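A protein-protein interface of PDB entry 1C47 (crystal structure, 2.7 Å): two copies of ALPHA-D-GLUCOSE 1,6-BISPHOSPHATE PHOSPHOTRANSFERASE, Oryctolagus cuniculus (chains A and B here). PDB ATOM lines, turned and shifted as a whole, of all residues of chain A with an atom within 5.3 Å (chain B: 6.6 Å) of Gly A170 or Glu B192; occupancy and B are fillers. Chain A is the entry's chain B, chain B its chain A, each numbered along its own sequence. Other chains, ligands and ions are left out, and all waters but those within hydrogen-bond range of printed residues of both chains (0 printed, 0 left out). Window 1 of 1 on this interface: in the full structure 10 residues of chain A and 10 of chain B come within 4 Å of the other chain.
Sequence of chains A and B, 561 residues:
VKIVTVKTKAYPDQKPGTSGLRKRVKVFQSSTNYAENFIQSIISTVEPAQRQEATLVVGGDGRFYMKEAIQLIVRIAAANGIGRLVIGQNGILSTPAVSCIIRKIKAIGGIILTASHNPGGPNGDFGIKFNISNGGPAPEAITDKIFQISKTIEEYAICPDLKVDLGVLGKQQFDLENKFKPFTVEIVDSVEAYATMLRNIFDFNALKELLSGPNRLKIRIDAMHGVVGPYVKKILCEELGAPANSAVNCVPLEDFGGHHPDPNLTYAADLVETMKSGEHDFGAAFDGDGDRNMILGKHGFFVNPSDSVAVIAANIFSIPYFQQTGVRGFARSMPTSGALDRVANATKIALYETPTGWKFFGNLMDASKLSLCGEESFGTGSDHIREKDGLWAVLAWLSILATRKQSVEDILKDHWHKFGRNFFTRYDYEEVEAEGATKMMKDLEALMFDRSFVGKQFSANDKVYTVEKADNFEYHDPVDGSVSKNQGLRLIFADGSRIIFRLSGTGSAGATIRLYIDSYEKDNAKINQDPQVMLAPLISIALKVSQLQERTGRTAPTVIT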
ATOM      1  N   VAL A 168      25.079  -0.520  -4.437  1.00  0.00           N
ATOM      2  CA  VAL A 168      25.077  -0.159  -3.013  1.00  0.00           C
ATOM      3  C   VAL A 168      23.707   0.470  -2.514  1.00  0.00           C
ATOM      4  O   VAL A 168      23.178   1.426  -3.087  1.00  0.00           O
ATOM      5  CB  VAL A 168      26.299   0.753  -2.763  1.00  0.00           C
ATOM      6  CG1 VAL A 168      25.922   2.226  -2.412  1.00  0.00           C
ATOM      7  CG2 VAL A 168      27.166   0.131  -1.695  1.00  0.00           C
ATOM      8  N   LEU A 169      23.149  -0.068  -1.457  1.00  0.00           N
ATOM      9  CA  LEU A 169      21.817   0.432  -0.912  1.00  0.00           C
ATOM     10  C   LEU A 169      21.879   1.827  -0.246  1.00  0.00           C
ATOM     11  O   LEU A 169      22.872   2.178   0.351  1.00  0.00           O
ATOM     12  CB  LEU A 169      21.319  -0.544   0.163  1.00  0.00           C
ATOM     13  CG  LEU A 169      20.072  -1.339  -0.123  1.00  0.00           C
ATOM     14  CD1 LEU A 169      20.183  -2.048  -1.469  1.00  0.00           C
ATOM     15  CD2 LEU A 169      19.843  -2.357   0.979  1.00  0.00           C
ATOM     16  N   GLY A 170      20.812   2.604  -0.312  1.00  0.00           N
ATOM     17  CA  GLY A 170      20.853   3.886   0.348  1.00  0.00           C
ATOM     18  C   GLY A 170      20.666   5.102  -0.559  1.00  0.00           C
ATOM     19  O   GLY A 170      20.471   5.004  -1.711  1.00  0.00           O
ATOM     20  N   LYS A 171      20.776   6.290   0.031  1.00  0.00           N
ATOM     21  CA  LYS A 171      20.586   7.543  -0.720  1.00  0.00           C
ATOM     22  C   LYS A 171      21.909   8.152  -1.212  1.00  0.00           C
ATOM     23  O   LYS A 171      22.878   8.173  -0.518  1.00  0.00           O
ATOM     24  CB  LYS A 171      19.904   8.531   0.199  1.00  0.00           C
ATOM     25  CG  LYS A 171      19.429   9.751  -0.483  1.00  0.00           C
ATOM     26  CD  LYS A 171      18.675  10.647   0.493  1.00  0.00           C
ATOM     27  CE  LYS A 171      17.134  10.327   0.482  1.00  0.00           C
ATOM     28  NZ  LYS A 171      16.853   8.964   0.957  1.00  0.00           N
ATOM     29  N   GLN A 172      21.927   8.608  -2.472  1.00  0.00           N
ATOM     30  CA  GLN A 172      23.136   9.252  -3.044  1.00  0.00           C
ATOM     31  C   GLN A 172      22.775  10.637  -3.523  1.00  0.00           C
ATOM     32  O   GLN A 172      21.790  10.839  -4.303  1.00  0.00           O
ATOM     33  CB  GLN A 172      23.679   8.443  -4.201  1.00  0.00           C
ATOM     34  CG  GLN A 172      24.413   7.212  -3.750  1.00  0.00           C
ATOM     35  CD  GLN A 172      24.780   6.274  -4.886  1.00  0.00           C
ATOM     36  OE1 GLN A 172      25.598   6.597  -5.773  1.00  0.00           O
ATOM     37  NE2 GLN A 172      24.195   5.062  -4.907  1.00  0.00           N
ATOM     38  N   VAL A 185      19.258  10.175  -5.535  1.00  0.00           N
ATOM     39  CA  VAL A 185      19.043   8.801  -6.081  1.00  0.00           C
ATOM     40  C   VAL A 185      18.820   7.849  -4.941  1.00  0.00           C
ATOM     41  O   VAL A 185      19.626   7.703  -4.094  1.00  0.00           O
ATOM     42  CB  VAL A 185      20.261   8.349  -6.917  1.00  0.00           C
ATOM     43  CG1 VAL A 185      20.138   6.901  -7.298  1.00  0.00           C
ATOM     44  CG2 VAL A 185      20.366   9.210  -8.162  1.00  0.00           C
ATOM     45  N   GLU A 186      17.716   7.221  -4.873  1.00  0.00           N
ATOM     46  CA  GLU A 186      17.493   6.288  -3.749  1.00  0.00           C
ATOM     47  C   GLU A 186      17.506   4.796  -4.182  1.00  0.00           C
ATOM     48  O   GLU A 186      16.547   4.274  -4.766  1.00  0.00           O
ATOM     49  CB  GLU A 186      16.161   6.576  -3.087  1.00  0.00           C
ATOM     50  CG  GLU A 186      16.300   6.833  -1.701  1.00  0.00           C
ATOM     51  CD  GLU A 186      15.090   7.208  -1.089  1.00  0.00           C
ATOM     52  OE1 GLU A 186      14.839   8.418  -0.980  1.00  0.00           O
ATOM     53  OE2 GLU A 186      14.366   6.323  -0.683  1.00  0.00           O
ATOM     54  N   ILE A 187      18.591   4.107  -3.855  1.00  0.00           N
ATOM     55  CA  ILE A 187      18.666   2.746  -4.214  1.00  0.00           C
ATOM     56  C   ILE A 187      17.984   1.839  -3.180  1.00  0.00           C
ATOM     57  O   ILE A 187      18.414   1.688  -2.085  1.00  0.00           O
ATOM     58  CB  ILE A 187      20.091   2.392  -4.507  1.00  0.00           C
ATOM     59  CG1 ILE A 187      20.575   3.282  -5.669  1.00  0.00           C
ATOM     60  CG2 ILE A 187      20.249   0.889  -4.805  1.00  0.00           C
ATOM     61  CD1 ILE A 187      21.888   2.793  -6.335  1.00  0.00           C
ATOM     62  N   LYS B 104      18.335  10.009  13.412  1.00  0.00           N
ATOM     63  CA  LYS B 104      17.700  10.171  12.056  1.00  0.00           C
ATOM     64  C   LYS B 104      16.151  10.062  12.091  1.00  0.00           C
ATOM     65  O   LYS B 104      15.418  10.990  11.673  1.00  0.00           O
ATOM     66  CB  LYS B 104      18.283   9.102  11.159  1.00  0.00           C
ATOM     67  CG  LYS B 104      17.675   9.037   9.761  1.00  0.00           C
ATOM     68  CD  LYS B 104      18.326   7.879   8.972  1.00  0.00           C
ATOM     69  CE  LYS B 104      17.457   7.492   7.781  1.00  0.00           C
ATOM     70  NZ  LYS B 104      18.100   6.431   7.021  1.00  0.00           N
ATOM     71  N   VAL B 188      15.414  -3.284   9.439  1.00  0.00           N
ATOM     72  CA  VAL B 188      16.165  -2.438   8.545  1.00  0.00           C
ATOM     73  C   VAL B 188      17.601  -3.015   8.208  1.00  0.00           C
ATOM     74  O   VAL B 188      18.213  -3.733   8.972  1.00  0.00           O
ATOM     75  CB  VAL B 188      16.295  -1.074   9.195  1.00  0.00           C
ATOM     76  CG1 VAL B 188      17.103  -0.071   8.302  1.00  0.00           C
ATOM     77  CG2 VAL B 188      14.940  -0.525   9.452  1.00  0.00           C
ATOM     78  N   ASP B 189      18.129  -2.736   7.009  1.00  0.00           N
ATOM     79  CA  ASP B 189      19.510  -3.208   6.648  1.00  0.00           C
ATOM     80  C   ASP B 189      20.521  -2.697   7.700  1.00  0.00           C
ATOM     81  O   ASP B 189      20.466  -1.573   8.136  1.00  0.00           O
ATOM     82  CB  ASP B 189      19.902  -2.623   5.274  1.00  0.00           C
ATOM     83  CG  ASP B 189      21.164  -3.204   4.738  1.00  0.00           C
ATOM     84  OD1 ASP B 189      21.226  -4.437   4.613  1.00  0.00           O
ATOM     85  OD2 ASP B 189      22.093  -2.447   4.419  1.00  0.00           O
ATOM     86  N   SER B 190      21.430  -3.504   8.112  1.00  0.00           N
ATOM     87  CA  SER B 190      22.422  -3.067   9.156  1.00  0.00           C
ATOM     88  C   SER B 190      23.326  -1.966   8.732  1.00  0.00           C
ATOM     89  O   SER B 190      23.657  -1.102   9.524  1.00  0.00           O
ATOM     90  CB  SER B 190      23.293  -4.242   9.586  1.00  0.00           C
ATOM     91  OG  SER B 190      22.521  -5.416   9.996  1.00  0.00           O
ATOM     92  N   VAL B 191      23.694  -1.880   7.475  1.00  0.00           N
ATOM     93  CA  VAL B 191      24.664  -0.774   7.067  1.00  0.00           C
ATOM     94  C   VAL B 191      24.018   0.464   6.382  1.00  0.00           C
ATOM     95  O   VAL B 191      24.481   1.560   6.568  1.00  0.00           O
ATOM     96  CB  VAL B 191      25.677  -1.366   6.155  1.00  0.00           C
ATOM     97  CG1 VAL B 191      26.739  -0.368   5.841  1.00  0.00           C
ATOM     98  CG2 VAL B 191      26.235  -2.660   6.780  1.00  0.00           C
ATOM     99  N   GLU B 192      22.871   0.294   5.591  1.00  0.00           N
ATOM    100  CA  GLU B 192      22.188   1.474   4.797  1.00  0.00           C
ATOM    101  C   GLU B 192      22.223   2.894   5.484  1.00  0.00           C
ATOM    102  O   GLU B 192      22.987   3.751   5.112  1.00  0.00           O
ATOM    103  CB  GLU B 192      20.743   1.104   4.518  1.00  0.00           C
ATOM    104  CG  GLU B 192      20.098   2.092   3.602  1.00  0.00           C
ATOM    105  CD  GLU B 192      19.178   3.080   4.282  1.00  0.00           C
ATOM    106  OE1 GLU B 192      18.235   2.648   4.996  1.00  0.00           O
ATOM    107  OE2 GLU B 192      19.382   4.289   4.090  1.00  0.00           O
ATOM    108  N   ALA B 193      21.342   3.149   6.510  1.00  0.00           N
ATOM    109  CA  ALA B 193      21.299   4.504   7.184  1.00  0.00           C
ATOM    110  C   ALA B 193      22.707   5.008   7.624  1.00  0.00           C
ATOM    111  O   ALA B 193      23.025   6.146   7.466  1.00  0.00           O
ATOM    112  CB  ALA B 193      20.432   4.428   8.403  1.00  0.00           C
ATOM    113  N   TYR B 194      23.539   4.110   8.114  1.00  0.00           N
ATOM    114  CA  TYR B 194      24.855   4.471   8.510  1.00  0.00           C
ATOM    115  C   TYR B 194      25.758   4.872   7.254  1.00  0.00           C
ATOM    116  O   TYR B 194      26.541   5.874   7.272  1.00  0.00           O
ATOM    117  CB  TYR B 194      25.456   3.291   9.270  1.00  0.00           C
ATOM    118  CG  TYR B 194      26.859   3.497   9.716  1.00  0.00           C
ATOM    119  CD1 TYR B 194      27.898   2.971   8.953  1.00  0.00           C
ATOM    120  CD2 TYR B 194      27.116   4.194  10.895  1.00  0.00           C
ATOM    121  CE1 TYR B 194      29.228   3.139   9.374  1.00  0.00           C
ATOM    122  CE2 TYR B 194      28.405   4.371  11.322  1.00  0.00           C
ATOM    123  CZ  TYR B 194      29.473   3.837  10.533  1.00  0.00           C
ATOM    124  OH  TYR B 194      30.750   4.023  10.914  1.00  0.00           O
ATOM    125  N   ALA B 195      25.666   4.120   6.164  1.00  0.00           N
ATOM    126  CA  ALA B 195      26.472   4.444   4.952  1.00  0.00           C
ATOM    127  C   ALA B 195      26.033   5.808   4.356  1.00  0.00           C
ATOM    128  O   ALA B 195      26.842   6.620   3.934  1.00  0.00           O
ATOM    129  CB  ALA B 195      26.220   3.359   3.870  1.00  0.00           C
ATOM    130  N   THR B 196      24.735   6.074   4.329  1.00  0.00           N
ATOM    131  CA  THR B 196      24.259   7.361   3.815  1.00  0.00           C
ATOM    132  C   THR B 196      24.815   8.499   4.651  1.00  0.00           C
ATOM    133  O   THR B 196      25.261   9.525   4.137  1.00  0.00           O
ATOM    134  CB  THR B 196      22.733   7.396   3.852  1.00  0.00           C
ATOM    135  OG1 THR B 196      22.293   6.330   3.021  1.00  0.00           O
ATOM    136  CG2 THR B 196      22.169   8.726   3.352  1.00  0.00           C
ATOM    137  N   MET B 197      24.832   8.333   5.982  1.00  0.00           N
ATOM    138  CA  MET B 197      25.414   9.397   6.915  1.00  0.00           C
ATOM    139  C   MET B 197      26.895   9.644   6.646  1.00  0.00           C
ATOM    140  O   MET B 197      27.336  10.777   6.555  1.00  0.00           O
ATOM    141  CB  MET B 197      25.248   8.944   8.361  1.00  0.00           C
ATOM    142  CG  MET B 197      25.827   9.912   9.370  1.00  0.00           C
ATOM    143  SD  MET B 197      26.068   9.144  11.045  1.00  0.00           S
ATOM    144  CE  MET B 197      27.087   7.751  10.580  1.00  0.00           C
ATOM    145  N   ARG B 199      28.419   8.954   3.798  1.00  0.00           N
ATOM    146  CA  ARG B 199      28.470   9.441   2.411  1.00  0.00           C
ATOM    147  C   ARG B 199      28.295  10.963   2.356  1.00  0.00           C
ATOM    148  O   ARG B 199      28.802  11.639   1.417  1.00  0.00           O
ATOM    149  CB  ARG B 199      27.392   8.752   1.643  1.00  0.00           C
ATOM    150  CG  ARG B 199      27.547   8.806   0.162  1.00  0.00           C
ATOM    151  CD  ARG B 199      27.163   7.421  -0.467  1.00  0.00           C
ATOM    152  NE  ARG B 199      25.854   7.016  -0.077  1.00  0.00           N
ATOM    153  CZ  ARG B 199      25.656   5.817   0.295  1.00  0.00           C
ATOM    154  NH1 ARG B 199      26.646   4.936   0.321  1.00  0.00           N
ATOM    155  NH2 ARG B 199      24.408   5.426   0.671  1.00  0.00           N
ATOM    156  N   TYR B 231      30.023  -3.822   7.977  1.00  0.00           N
ATOM    157  CA  TYR B 231      30.291  -2.383   7.654  1.00  0.00           C
ATOM    158  C   TYR B 231      31.639  -2.172   6.874  1.00  0.00           C
ATOM    159  O   TYR B 231      31.737  -1.310   6.032  1.00  0.00           O
ATOM    160  CB  TYR B 231      30.303  -1.583   8.907  1.00  0.00           C
ATOM    161  CG  TYR B 231      28.947  -1.607   9.703  1.00  0.00           C
ATOM    162  CD1 TYR B 231      28.702  -2.609  10.643  1.00  0.00           C
ATOM    163  CD2 TYR B 231      28.009  -0.607   9.509  1.00  0.00           C
ATOM    164  CE1 TYR B 231      27.577  -2.590  11.364  1.00  0.00           C
ATOM    165  CE2 TYR B 231      26.883  -0.599  10.240  1.00  0.00           C
ATOM    166  CZ  TYR B 231      26.659  -1.587  11.160  1.00  0.00           C
ATOM    167  OH  TYR B 231      25.452  -1.575  11.900  1.00  0.00           O
ATOM    168  N   LYS B 234      30.803  -3.888   3.123  1.00  0.00           N
ATOM    169  CA  LYS B 234      29.870  -3.047   2.341  1.00  0.00           C
ATOM    170  C   LYS B 234      30.407  -1.647   2.011  1.00  0.00           C
ATOM    171  O   LYS B 234      30.310  -1.186   0.866  1.00  0.00           O
ATOM    172  CB  LYS B 234      28.553  -2.946   3.054  1.00  0.00           C
ATOM    173  CG  LYS B 234      27.647  -4.159   2.762  1.00  0.00           C
ATOM    174  CD  LYS B 234      26.269  -3.885   3.289  1.00  0.00           C
ATOM    175  CE  LYS B 234      25.294  -4.908   2.736  1.00  0.00           C
ATOM    176  NZ  LYS B 234      23.925  -4.609   3.201  1.00  0.00           N
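The backbone carbonyl oxygen of Lys A171 sits at hydrogen-bond distance from the guanidinium group of Arg B199 (3.2 Å). OG1 of Thr B196 sits at hydrogen-bond distance from N of Lys A171, 3.4 Å away.
The side-chain carboxylate (OD2) of Asp B189 sits at hydrogen-bond distance from the backbone NH (N) of Glu B192, at 3.1 Å. O of Glu B192 lies within hydrogen-bond range of OG1 of Thr B196 (3.4 Å). O of Gly A170 lies within hydrogen-bond range of N of Ile A187, at 3.0 Å. OE2 of Glu B192 lies within salt-bridge range of NZ of Lys B104. The side-chain hydroxyl of Thr B196 is in hydrogen-bond range of the guanidinium group of Arg B199 (3.3 Å). The backbone carbonyl oxygen of Gln A172 is in hydrogen-bond range of the backbone NH of Val A185, 2.9 Å away.
Val A168 touches Arg B199 (CG1 to NH1, 3.9 Å). Arg B199 touches Leu A169. Gly A170 touches Glu B192. Gly A170 touches Thr B196. CA of Gly A170 touches NH2 of Arg B199, at 3.9 Å. Arg B199 touches Gln A172 (NE to CG, 3.95 Å).
Of the printed residues of chain B, Leu A169 touches Arg B199. Printed residues of chain B within 4 Å of Gly A170: Glu B192 (3.8 Å), Thr B196 (3.9 Å) and Arg B199 (3.9 Å). Of the printed residues of chain B, Lys A171 touches Thr B196 (3.4 Å) and Arg B199 (3.2 Å). Of the printed residues of chain A, Glu B192 touches Gly A170. Of the printed residues of chain A, Thr B196 touches Gly A170 and Lys A171. Of the printed residues of chain A, Arg B199 touches Val A168, Leu A169, Gly A170, Lys A171 and Gln A172. The nearest residue of chain B that does not touch Gly A170 is Ala B193 (6.2 Å). The nearest residue of chain A that does not touch Glu B192 is Leu A169 (4.2 Å). The nearest printed residue of chain B that does not touch Lys A171 is Glu B192 (4.7 Å).
Printed residues of chain B that touch a printed residue of chain A: Glu B192, Thr B196 and Arg B199. Of the 8 printed residues of chain A, 5 touch a printed residue of chain B. Printed residues of chain A that touch a printed residue of chain B: Val A168, Leu A169, Gly A170, Lys A171 and Gln A172.
No position is printed for both chains. Of the 8 pairs that touch across the chains among the printed residues, none has its exchanged pair printed and touching as well.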
